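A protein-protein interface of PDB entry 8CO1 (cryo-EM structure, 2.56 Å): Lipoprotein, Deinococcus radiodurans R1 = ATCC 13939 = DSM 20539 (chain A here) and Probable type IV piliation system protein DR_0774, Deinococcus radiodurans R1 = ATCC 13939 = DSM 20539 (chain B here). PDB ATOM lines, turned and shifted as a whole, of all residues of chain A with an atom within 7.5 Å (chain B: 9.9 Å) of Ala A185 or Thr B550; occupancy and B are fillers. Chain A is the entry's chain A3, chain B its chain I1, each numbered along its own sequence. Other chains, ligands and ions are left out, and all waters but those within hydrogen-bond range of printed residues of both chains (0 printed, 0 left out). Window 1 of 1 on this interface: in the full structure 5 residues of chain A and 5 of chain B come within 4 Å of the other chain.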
ATOM      1  N   GLY A  28      16.944 -37.256   3.372  1.00  0.00           N
ATOM      2  CA  GLY A  28      17.243 -36.050   2.622  1.00  0.00           C
ATOM      3  C   GLY A  28      16.674 -36.051   1.216  1.00  0.00           C
ATOM      4  O   GLY A  28      16.877 -36.994   0.455  1.00  0.00           O
ATOM      5  N   VAL A  30      15.671 -33.398  -2.321  1.00  0.00           N
ATOM      6  CA  VAL A  30      15.843 -32.141  -3.038  1.00  0.00           C
ATOM      7  C   VAL A  30      14.627 -31.944  -3.933  1.00  0.00           C
ATOM      8  O   VAL A  30      14.234 -32.858  -4.663  1.00  0.00           O
ATOM      9  CB  VAL A  30      17.142 -32.128  -3.863  1.00  0.00           C
ATOM     10  CG1 VAL A  30      17.249 -30.841  -4.654  1.00  0.00           C
ATOM     11  CG2 VAL A  30      18.344 -32.308  -2.963  1.00  0.00           C
ATOM     12  N   GLY A  84      10.368 -28.333   2.846  1.00  0.00           N
ATOM     13  CA  GLY A  84      10.971 -29.570   3.288  1.00  0.00           C
ATOM     14  C   GLY A  84      12.200 -29.998   2.522  1.00  0.00           C
ATOM     15  O   GLY A  84      12.736 -31.076   2.801  1.00  0.00           O
ATOM     16  N   SER A  85      12.669 -29.194   1.576  1.00  0.00           N
ATOM     17  CA  SER A  85      13.782 -29.557   0.716  1.00  0.00           C
ATOM     18  C   SER A  85      15.108 -29.105   1.317  1.00  0.00           C
ATOM     19  O   SER A  85      15.159 -28.279   2.228  1.00  0.00           O
ATOM     20  CB  SER A  85      13.602 -28.941  -0.671  1.00  0.00           C
ATOM     21  OG  SER A  85      14.670 -29.288  -1.529  1.00  0.00           O
ATOM     22  N   GLU A  86      16.191 -29.675   0.800  1.00  0.00           N
ATOM     23  CA  GLU A  86      17.524 -29.236   1.174  1.00  0.00           C
ATOM     24  C   GLU A  86      17.913 -28.002   0.367  1.00  0.00           C
ATOM     25  O   GLU A  86      17.206 -27.572  -0.546  1.00  0.00           O
ATOM     26  CB  GLU A  86      18.543 -30.348   0.950  1.00  0.00           C
ATOM     27  CG  GLU A  86      18.217 -31.655   1.611  1.00  0.00           C
ATOM     28  CD  GLU A  86      19.433 -32.537   1.725  1.00  0.00           C
ATOM     29  OE1 GLU A  86      20.520 -31.993   1.989  1.00  0.00           O
ATOM     30  OE2 GLU A  86      19.309 -33.765   1.549  1.00  0.00           O
ATOM     31  N   ALA A  87      19.055 -27.420   0.712  1.00  0.00           N
ATOM     32  CA  ALA A  87      19.666 -26.429  -0.152  1.00  0.00           C
ATOM     33  C   ALA A  87      20.432 -27.126  -1.269  1.00  0.00           C
ATOM     34  O   ALA A  87      20.849 -28.280  -1.147  1.00  0.00           O
ATOM     35  CB  ALA A  87      20.597 -25.514   0.640  1.00  0.00           C
ATOM     36  N   VAL A  88      20.609 -26.414  -2.379  1.00  0.00           N
ATOM     37  CA  VAL A  88      21.282 -26.976  -3.541  1.00  0.00           C
ATOM     38  C   VAL A  88      22.005 -25.851  -4.262  1.00  0.00           C
ATOM     39  O   VAL A  88      21.584 -24.693  -4.221  1.00  0.00           O
ATOM     40  CB  VAL A  88      20.285 -27.709  -4.472  1.00  0.00           C
ATOM     41  CG1 VAL A  88      19.458 -26.721  -5.265  1.00  0.00           C
ATOM     42  CG2 VAL A  88      21.008 -28.665  -5.392  1.00  0.00           C
ATOM     43  N   THR A  89      23.120 -26.196  -4.901  1.00  0.00           N
ATOM     44  CA  THR A  89      23.894 -25.261  -5.707  1.00  0.00           C
ATOM     45  C   THR A  89      23.979 -25.789  -7.129  1.00  0.00           C
ATOM     46  O   THR A  89      24.390 -26.932  -7.346  1.00  0.00           O
ATOM     47  CB  THR A  89      25.297 -25.059  -5.135  1.00  0.00           C
ATOM     48  OG1 THR A  89      25.203 -24.477  -3.832  1.00  0.00           O
ATOM     49  CG2 THR A  89      26.097 -24.138  -6.025  1.00  0.00           C
ATOM     50  N   TYR A 120      23.145 -20.485  -5.703  1.00  0.00           N
ATOM     51  CA  TYR A 120      22.710 -21.095  -4.455  1.00  0.00           C
ATOM     52  C   TYR A 120      21.201 -20.966  -4.298  1.00  0.00           C
ATOM     53  O   TYR A 120      20.656 -19.860  -4.358  1.00  0.00           O
ATOM     54  CB  TYR A 120      23.416 -20.437  -3.270  1.00  0.00           C
ATOM     55  CG  TYR A 120      23.288 -21.194  -1.973  1.00  0.00           C
ATOM     56  CD1 TYR A 120      23.703 -22.511  -1.874  1.00  0.00           C
ATOM     57  CD2 TYR A 120      22.758 -20.586  -0.846  1.00  0.00           C
ATOM     58  CE1 TYR A 120      23.593 -23.204  -0.692  1.00  0.00           C
ATOM     59  CE2 TYR A 120      22.641 -21.272   0.342  1.00  0.00           C
ATOM     60  CZ  TYR A 120      23.061 -22.582   0.414  1.00  0.00           C
ATOM     61  OH  TYR A 120      22.953 -23.275   1.596  1.00  0.00           O
ATOM     62  N   SER A 123      17.300 -23.341   1.429  1.00  0.00           N
ATOM     63  CA  SER A 123      16.812 -24.666   1.807  1.00  0.00           C
ATOM     64  C   SER A 123      15.324 -24.836   1.534  1.00  0.00           C
ATOM     65  O   SER A 123      14.897 -25.875   1.020  1.00  0.00           O
ATOM     66  CB  SER A 123      17.108 -24.923   3.283  1.00  0.00           C
ATOM     67  OG  SER A 123      16.786 -26.254   3.638  1.00  0.00           O
ATOM     68  N   TYR A 125      13.028 -23.510   4.131  1.00  0.00           N
ATOM     69  CA  TYR A 125      12.497 -23.436   5.480  1.00  0.00           C
ATOM     70  C   TYR A 125      12.339 -21.967   5.845  1.00  0.00           C
ATOM     71  O   TYR A 125      12.602 -21.073   5.038  1.00  0.00           O
ATOM     72  CB  TYR A 125      13.404 -24.156   6.483  1.00  0.00           C
ATOM     73  CG  TYR A 125      13.430 -25.663   6.357  1.00  0.00           C
ATOM     74  CD1 TYR A 125      14.141 -26.284   5.347  1.00  0.00           C
ATOM     75  CD2 TYR A 125      12.756 -26.462   7.263  1.00  0.00           C
ATOM     76  CE1 TYR A 125      14.172 -27.658   5.239  1.00  0.00           C
ATOM     77  CE2 TYR A 125      12.780 -27.832   7.162  1.00  0.00           C
ATOM     78  CZ  TYR A 125      13.489 -28.426   6.149  1.00  0.00           C
ATOM     79  OH  TYR A 125      13.514 -29.795   6.047  1.00  0.00           O
ATOM     80  N   SER A 135      20.575 -20.368   4.351  1.00  0.00           N
ATOM     81  CA  SER A 135      19.644 -21.425   4.704  1.00  0.00           C
ATOM     82  C   SER A 135      19.607 -21.578   6.216  1.00  0.00           C
ATOM     83  O   SER A 135      20.586 -21.293   6.909  1.00  0.00           O
ATOM     84  CB  SER A 135      20.037 -22.756   4.058  1.00  0.00           C
ATOM     85  OG  SER A 135      19.573 -22.831   2.724  1.00  0.00           O
ATOM     86  N   CYS A 136      18.460 -22.022   6.721  1.00  0.00           N
ATOM     87  CA  CYS A 136      18.326 -22.295   8.142  1.00  0.00           C
ATOM     88  C   CYS A 136      19.200 -23.476   8.541  1.00  0.00           C
ATOM     89  O   CYS A 136      19.475 -24.373   7.740  1.00  0.00           O
ATOM     90  CB  CYS A 136      16.870 -22.591   8.495  1.00  0.00           C
ATOM     91  SG  CYS A 136      15.681 -21.388   7.884  1.00  0.00           S
ATOM     92  N   GLN A 137      19.646 -23.464   9.798  1.00  0.00           N
ATOM     93  CA  GLN A 137      20.397 -24.599  10.322  1.00  0.00           C
ATOM     94  C   GLN A 137      19.548 -25.862  10.340  1.00  0.00           C
ATOM     95  O   GLN A 137      20.017 -26.940   9.958  1.00  0.00           O
ATOM     96  CB  GLN A 137      20.903 -24.300  11.731  1.00  0.00           C
ATOM     97  CG  GLN A 137      21.763 -23.070  11.863  1.00  0.00           C
ATOM     98  CD  GLN A 137      23.231 -23.409  11.811  1.00  0.00           C
ATOM     99  OE1 GLN A 137      23.753 -23.786  10.762  1.00  0.00           O
ATOM    100  NE2 GLN A 137      23.896 -23.335  12.957  1.00  0.00           N
ATOM    101  N   GLY A 138      18.298 -25.748  10.781  1.00  0.00           N
ATOM    102  CA  GLY A 138      17.399 -26.880  10.885  1.00  0.00           C
ATOM    103  C   GLY A 138      16.969 -27.232  12.293  1.00  0.00           C
ATOM    104  O   GLY A 138      16.206 -28.189  12.463  1.00  0.00           O
ATOM    105  N   ASN A 139      17.426 -26.500  13.305  1.00  0.00           N
ATOM    106  CA  ASN A 139      17.109 -26.804  14.697  1.00  0.00           C
ATOM    107  C   ASN A 139      16.808 -25.529  15.471  1.00  0.00           C
ATOM    108  O   ASN A 139      17.282 -25.337  16.595  1.00  0.00           O
ATOM    109  CB  ASN A 139      18.245 -27.584  15.354  1.00  0.00           C
ATOM    110  CG  ASN A 139      19.593 -26.922  15.156  1.00  0.00           C
ATOM    111  OD1 ASN A 139      19.685 -25.825  14.609  1.00  0.00           O
ATOM    112  ND2 ASN A 139      20.648 -27.590  15.602  1.00  0.00           N
ATOM    113  N   ILE A 143      11.499 -23.253  13.421  1.00  0.00           N
ATOM    114  CA  ILE A 143      11.622 -23.463  11.989  1.00  0.00           C
ATOM    115  C   ILE A 143      10.348 -24.081  11.428  1.00  0.00           C
ATOM    116  O   ILE A 143       9.739 -24.974  12.034  1.00  0.00           O
ATOM    117  CB  ILE A 143      12.862 -24.328  11.700  1.00  0.00           C
ATOM    118  CG1 ILE A 143      13.197 -24.310  10.212  1.00  0.00           C
ATOM    119  CG2 ILE A 143      12.685 -25.746  12.226  1.00  0.00           C
ATOM    120  CD1 ILE A 143      14.520 -24.942   9.892  1.00  0.00           C
ATOM    121  N   PHE A 183      24.855 -29.961  -6.810  1.00  0.00           N
ATOM    122  CA  PHE A 183      24.971 -30.803  -5.629  1.00  0.00           C
ATOM    123  C   PHE A 183      24.187 -30.166  -4.492  1.00  0.00           C
ATOM    124  O   PHE A 183      24.051 -28.942  -4.428  1.00  0.00           O
ATOM    125  CB  PHE A 183      26.436 -31.002  -5.227  1.00  0.00           C
ATOM    126  CG  PHE A 183      27.125 -29.739  -4.803  1.00  0.00           C
ATOM    127  CD1 PHE A 183      27.443 -28.762  -5.725  1.00  0.00           C
ATOM    128  CD2 PHE A 183      27.457 -29.531  -3.479  1.00  0.00           C
ATOM    129  CE1 PHE A 183      28.072 -27.603  -5.335  1.00  0.00           C
ATOM    130  CE2 PHE A 183      28.087 -28.375  -3.084  1.00  0.00           C
ATOM    131  CZ  PHE A 183      28.395 -27.410  -4.014  1.00  0.00           C
ATOM    132  N   SER A 184      23.677 -31.001  -3.593  1.00  0.00           N
ATOM    133  CA  SER A 184      22.859 -30.515  -2.493  1.00  0.00           C
ATOM    134  C   SER A 184      23.750 -30.106  -1.324  1.00  0.00           C
ATOM    135  O   SER A 184      24.978 -30.083  -1.426  1.00  0.00           O
ATOM    136  CB  SER A 184      21.855 -31.574  -2.057  1.00  0.00           C
ATOM    137  OG  SER A 184      22.511 -32.624  -1.381  1.00  0.00           O
ATOM    138  N   ALA A 185      23.132 -29.781  -0.189  1.00  0.00           N
ATOM    139  CA  ALA A 185      23.899 -29.421   0.994  1.00  0.00           C
ATOM    140  C   ALA A 185      24.624 -30.616   1.594  1.00  0.00           C
ATOM    141  O   ALA A 185      25.544 -30.428   2.394  1.00  0.00           O
ATOM    142  CB  ALA A 185      22.987 -28.780   2.035  1.00  0.00           C
ATOM    143  N   ASN A 186      24.233 -31.834   1.231  1.00  0.00           N
ATOM    144  CA  ASN A 186      24.937 -33.042   1.626  1.00  0.00           C
ATOM    145  C   ASN A 186      25.874 -33.538   0.538  1.00  0.00           C
ATOM    146  O   ASN A 186      26.356 -34.671   0.617  1.00  0.00           O
ATOM    147  CB  ASN A 186      23.940 -34.140   1.998  1.00  0.00           C
ATOM    148  CG  ASN A 186      23.233 -33.868   3.307  1.00  0.00           C
ATOM    149  OD1 ASN A 186      23.651 -34.336   4.361  1.00  0.00           O
ATOM    150  ND2 ASN A 186      22.155 -33.108   3.245  1.00  0.00           N
ATOM    151  N   ASN A 187      26.126 -32.714  -0.482  1.00  0.00           N
ATOM    152  CA  ASN A 187      27.083 -33.012  -1.547  1.00  0.00           C
ATOM    153  C   ASN A 187      26.692 -34.266  -2.325  1.00  0.00           C
ATOM    154  O   ASN A 187      27.487 -35.190  -2.497  1.00  0.00           O
ATOM    155  CB  ASN A 187      28.503 -33.135  -0.990  1.00  0.00           C
ATOM    156  CG  ASN A 187      28.812 -32.087   0.057  1.00  0.00           C
ATOM    157  OD1 ASN A 187      28.456 -30.919  -0.094  1.00  0.00           O
ATOM    158  ND2 ASN A 187      29.481 -32.499   1.127  1.00  0.00           N
ATOM    159  N   VAL A 188      25.455 -34.291  -2.810  1.00  0.00           N
ATOM    160  CA  VAL A 188      25.007 -35.385  -3.668  1.00  0.00           C
ATOM    161  C   VAL A 188      24.531 -34.806  -4.995  1.00  0.00           C
ATOM    162  O   VAL A 188      23.955 -33.710  -5.025  1.00  0.00           O
ATOM    163  CB  VAL A 188      23.913 -36.228  -2.993  1.00  0.00           C
ATOM    164  CG1 VAL A 188      24.458 -36.906  -1.745  1.00  0.00           C
ATOM    165  CG2 VAL A 188      22.703 -35.386  -2.668  1.00  0.00           C
ATOM    166  N   GLY B 531      31.333 -35.040   8.743  1.00  0.00           N
ATOM    167  CA  GLY B 531      30.116 -34.896   7.960  1.00  0.00           C
ATOM    168  C   GLY B 531      28.815 -35.199   8.670  1.00  0.00           C
ATOM    169  O   GLY B 531      28.478 -36.362   8.909  1.00  0.00           O
ATOM    170  N   GLY B 532      28.058 -34.153   8.986  1.00  0.00           N
ATOM    171  CA  GLY B 532      26.807 -34.308   9.697  1.00  0.00           C
ATOM    172  C   GLY B 532      26.947 -34.288  11.205  1.00  0.00           C
ATOM    173  O   GLY B 532      26.041 -33.841  11.909  1.00  0.00           O
ATOM    174  N   PHE B 533      28.081 -34.753  11.713  1.00  0.00           N
ATOM    175  CA  PHE B 533      28.301 -34.934  13.139  1.00  0.00           C
ATOM    176  C   PHE B 533      29.010 -33.738  13.754  1.00  0.00           C
ATOM    177  O   PHE B 533      29.787 -33.043  13.099  1.00  0.00           O
ATOM    178  CB  PHE B 533      29.114 -36.197  13.397  1.00  0.00           C
ATOM    179  CG  PHE B 533      28.342 -37.451  13.185  1.00  0.00           C
ATOM    180  CD1 PHE B 533      27.618 -38.011  14.219  1.00  0.00           C
ATOM    181  CD2 PHE B 533      28.320 -38.062  11.951  1.00  0.00           C
ATOM    182  CE1 PHE B 533      26.899 -39.162  14.028  1.00  0.00           C
ATOM    183  CE2 PHE B 533      27.599 -39.214  11.754  1.00  0.00           C
ATOM    184  CZ  PHE B 533      26.889 -39.766  12.794  1.00  0.00           C
ATOM    185  N   PHE B 547      23.687 -34.659  15.444  1.00  0.00           N
ATOM    186  CA  PHE B 547      23.671 -34.981  14.025  1.00  0.00           C
ATOM    187  C   PHE B 547      22.771 -33.995  13.299  1.00  0.00           C
ATOM    188  O   PHE B 547      21.719 -33.607  13.812  1.00  0.00           O
ATOM    189  CB  PHE B 547      23.186 -36.404  13.774  1.00  0.00           C
ATOM    190  CG  PHE B 547      23.144 -36.776  12.326  1.00  0.00           C
ATOM    191  CD1 PHE B 547      24.285 -36.736  11.555  1.00  0.00           C
ATOM    192  CD2 PHE B 547      21.958 -37.158  11.731  1.00  0.00           C
ATOM    193  CE1 PHE B 547      24.247 -37.077  10.225  1.00  0.00           C
ATOM    194  CE2 PHE B 547      21.917 -37.500  10.399  1.00  0.00           C
ATOM    195  CZ  PHE B 547      23.064 -37.457   9.646  1.00  0.00           C
ATOM    196  N   ASN B 548      23.196 -33.584  12.112  1.00  0.00           N
ATOM    197  CA  ASN B 548      22.420 -32.675  11.270  1.00  0.00           C
ATOM    198  C   ASN B 548      22.166 -33.337   9.928  1.00  0.00           C
ATOM    199  O   ASN B 548      23.107 -33.485   9.127  1.00  0.00           O
ATOM    200  CB  ASN B 548      23.156 -31.350  11.082  1.00  0.00           C
ATOM    201  CG  ASN B 548      22.255 -30.249  10.588  1.00  0.00           C
ATOM    202  OD1 ASN B 548      21.193 -30.504  10.034  1.00  0.00           O
ATOM    203  ND2 ASN B 548      22.674 -29.012  10.788  1.00  0.00           N
ATOM    204  N   PRO B 549      20.934 -33.756   9.628  1.00  0.00           N
ATOM    205  CA  PRO B 549      20.673 -34.431   8.351  1.00  0.00           C
ATOM    206  C   PRO B 549      20.532 -33.492   7.168  1.00  0.00           C
ATOM    207  O   PRO B 549      20.408 -33.973   6.037  1.00  0.00           O
ATOM    208  CB  PRO B 549      19.351 -35.174   8.614  1.00  0.00           C
ATOM    209  CG  PRO B 549      19.051 -34.980  10.079  1.00  0.00           C
ATOM    210  CD  PRO B 549      19.736 -33.728  10.474  1.00  0.00           C
ATOM    211  N   THR B 550      20.548 -32.180   7.386  1.00  0.00           N
ATOM    212  CA  THR B 550      20.327 -31.216   6.319  1.00  0.00           C
ATOM    213  C   THR B 550      21.611 -30.657   5.725  1.00  0.00           C
ATOM    214  O   THR B 550      21.604 -30.225   4.570  1.00  0.00           O
ATOM    215  CB  THR B 550      19.469 -30.055   6.829  1.00  0.00           C
ATOM    216  OG1 THR B 550      20.062 -29.507   8.011  1.00  0.00           O
ATOM    217  CG2 THR B 550      18.072 -30.535   7.155  1.00  0.00           C
ATOM    218  N   GLN B 551      22.703 -30.648   6.476  1.00  0.00           N
ATOM    219  CA  GLN B 551      23.987 -30.142   6.020  1.00  0.00           C
ATOM    220  C   GLN B 551      25.028 -31.250   6.108  1.00  0.00           C
ATOM    221  O   GLN B 551      24.730 -32.382   6.490  1.00  0.00           O
ATOM    222  CB  GLN B 551      24.417 -28.928   6.843  1.00  0.00           C
ATOM    223  CG  GLN B 551      24.092 -27.603   6.201  1.00  0.00           C
ATOM    224  CD  GLN B 551      23.924 -26.495   7.215  1.00  0.00           C
ATOM    225  OE1 GLN B 551      24.536 -26.518   8.280  1.00  0.00           O
ATOM    226  NE2 GLN B 551      23.093 -25.514   6.888  1.00  0.00           N
ATOM    227  N   SER B 552      26.262 -30.912   5.747  1.00  0.00           N
ATOM    228  CA  SER B 552      27.358 -31.875   5.801  1.00  0.00           C
ATOM    229  C   SER B 552      28.671 -31.112   5.797  1.00  0.00           C
ATOM    230  O   SER B 552      28.931 -30.339   4.871  1.00  0.00           O
ATOM    231  CB  SER B 552      27.288 -32.842   4.627  1.00  0.00           C
ATOM    232  OG  SER B 552      28.243 -33.874   4.761  1.00  0.00           O
ATOM    233  N   PHE B 553      29.490 -31.323   6.823  1.00  0.00           N
ATOM    234  CA  PHE B 553      30.772 -30.645   6.928  1.00  0.00           C
ATOM    235  C   PHE B 553      31.750 -31.175   5.885  1.00  0.00           C
ATOM    236  O   PHE B 553      31.568 -32.247   5.305  1.00  0.00           O
ATOM    237  CB  PHE B 553      31.375 -30.836   8.320  1.00  0.00           C
ATOM    238  CG  PHE B 553      30.642 -30.114   9.412  1.00  0.00           C
ATOM    239  CD1 PHE B 553      30.698 -28.738   9.514  1.00  0.00           C
ATOM    240  CD2 PHE B 553      29.910 -30.820  10.350  1.00  0.00           C
ATOM    241  CE1 PHE B 553      30.031 -28.081  10.523  1.00  0.00           C
ATOM    242  CE2 PHE B 553      29.242 -30.168  11.359  1.00  0.00           C
ATOM    243  CZ  PHE B 553      29.302 -28.798  11.446  1.00  0.00           C
ATOM    244  N   LEU B 554      32.811 -30.406   5.660  1.00  0.00           N
ATOM    245  CA  LEU B 554      33.888 -30.791   4.760  1.00  0.00           C
ATOM    246  C   LEU B 554      35.066 -31.308   5.575  1.00  0.00           C
ATOM    247  O   LEU B 554      35.612 -30.580   6.410  1.00  0.00           O
ATOM    248  CB  LEU B 554      34.322 -29.613   3.894  1.00  0.00           C
ATOM    249  CG  LEU B 554      33.632 -29.417   2.548  1.00  0.00           C
ATOM    250  CD1 LEU B 554      34.423 -28.425   1.725  1.00  0.00           C
ATOM    251  CD2 LEU B 554      33.500 -30.732   1.816  1.00  0.00           C
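Of chain A, only Glu A86, Gln A137, Ala A185 and Asn A186 come within 4 Å of Thr B550. No residue of chain B comes within 4 Å of Ala A87. No residue of chain B comes within 4 Å of Ser A184. Asn A186 touches just these residues of chain B: Pro B549, Thr B550, Gln B551 and Ser B552. Of the printed residues of chain B, Cys A136 touches Gln B551 (3.9 Å). Of the printed residues of chain A, Ser B552 touches Ala A185 and Asn A186. Printed residues of chain B within 4 Å of Gln A137: Asn B548 (3.5 Å), Thr B550 (3.2 Å) and Gln B551 (3.8 Å). Printed residues of chain A within 4 Å of Pro B549: Asn A186 (3.4 Å). Of the printed residues of chain B, Glu A86 touches Thr B550. Phe B547 touches none of the printed residues of chain A. Ser A135 touches none of the printed residues of chain B. The nearest residue of chain B that does not touch Ala A185 is Phe B553 (6.0 Å). The nearest residue of chain A that does not touch Thr B550 is Gly A138 (4.7 Å). The nearest printed residue of chain A that does not touch Ser B552 is Asn A187 (4.1 Å).
The backbone NH (N) of Asn B548 is in hydrogen-bond range of the backbone carbonyl oxygen (O) of Gly B532 (2.9 Å). The side-chain amide oxygen (OD1) of Asn B548 sits at hydrogen-bond distance from the side-chain hydroxyl (OG1) of Thr B550, 2.5 Å away. The side-chain amide nitrogen (ND2) of Asn A186 sits close to the side-chain carboxylate (OE2) of Glu A86 (3.4 Å). The backbone NH (N) of Ala A185 is in hydrogen-bond range of the backbone carbonyl oxygen (O) of Ala A87, at 2.9 Å. The side-chain hydroxyl (OG) of Ser A184 lies close to the backbone NH (N) of Asn A186 (3.2 Å).
Among the printed residues, merely in contact across the chains: Ala A185 with Thr B550 (3.2 Å), Gln A137 with Gln B551 (3.8 Å), Asn A186 with Ser B552 (3.8 Å), Ala A185 with Gln B551 (3.8 Å) and Cys A136 with Gln B551 (3.9 Å).
Of the 11 printed residues of chain B, 5 touch a printed residue of chain A. Along chain B the printed residues that touch a printed residue of chain A span positions 548 to 552. Of the 23 printed residues of chain A, 5 touch a printed residue of chain B. Printed residues of chain A that touch a printed residue of chain B: Glu A86, Cys A136, Gln A137, Ala A185 and Asn A186. Hydrophobic or aromatic side chains of chain A within 4 Å of the printed part of chain B: Ala A185. Along chain A the printed residues that touch a printed residue of chain B span positions 86 to 186.
The side-chain amide nitrogen of Asn B548 is in hydrogen-bond range of the backbone carbonyl oxygen of Gln A137 (3.5 Å). O of Pro B549 lies within hydrogen-bond range of ND2 of Asn A186. The side-chain hydroxyl (OG1) of Thr B550 is in hydrogen-bond range of the backbone carbonyl oxygen (O) of Gln A137 (3.2 Å). The backbone carbonyl oxygen (O) of Thr B550 is in hydrogen-bond range of the side-chain amide nitrogen (ND2) of Asn A186. O of Gln B551 lies close to OD1 of Asn A186, 3.1 Å away. O of Ala A185 sits at hydrogen-bond distance from N of Ser B552, 3.5 Å away. The side-chain carboxylate (OE1) of Glu A86 sits close to the backbone carbonyl oxygen (O) of Thr B550 (3.3 Å).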
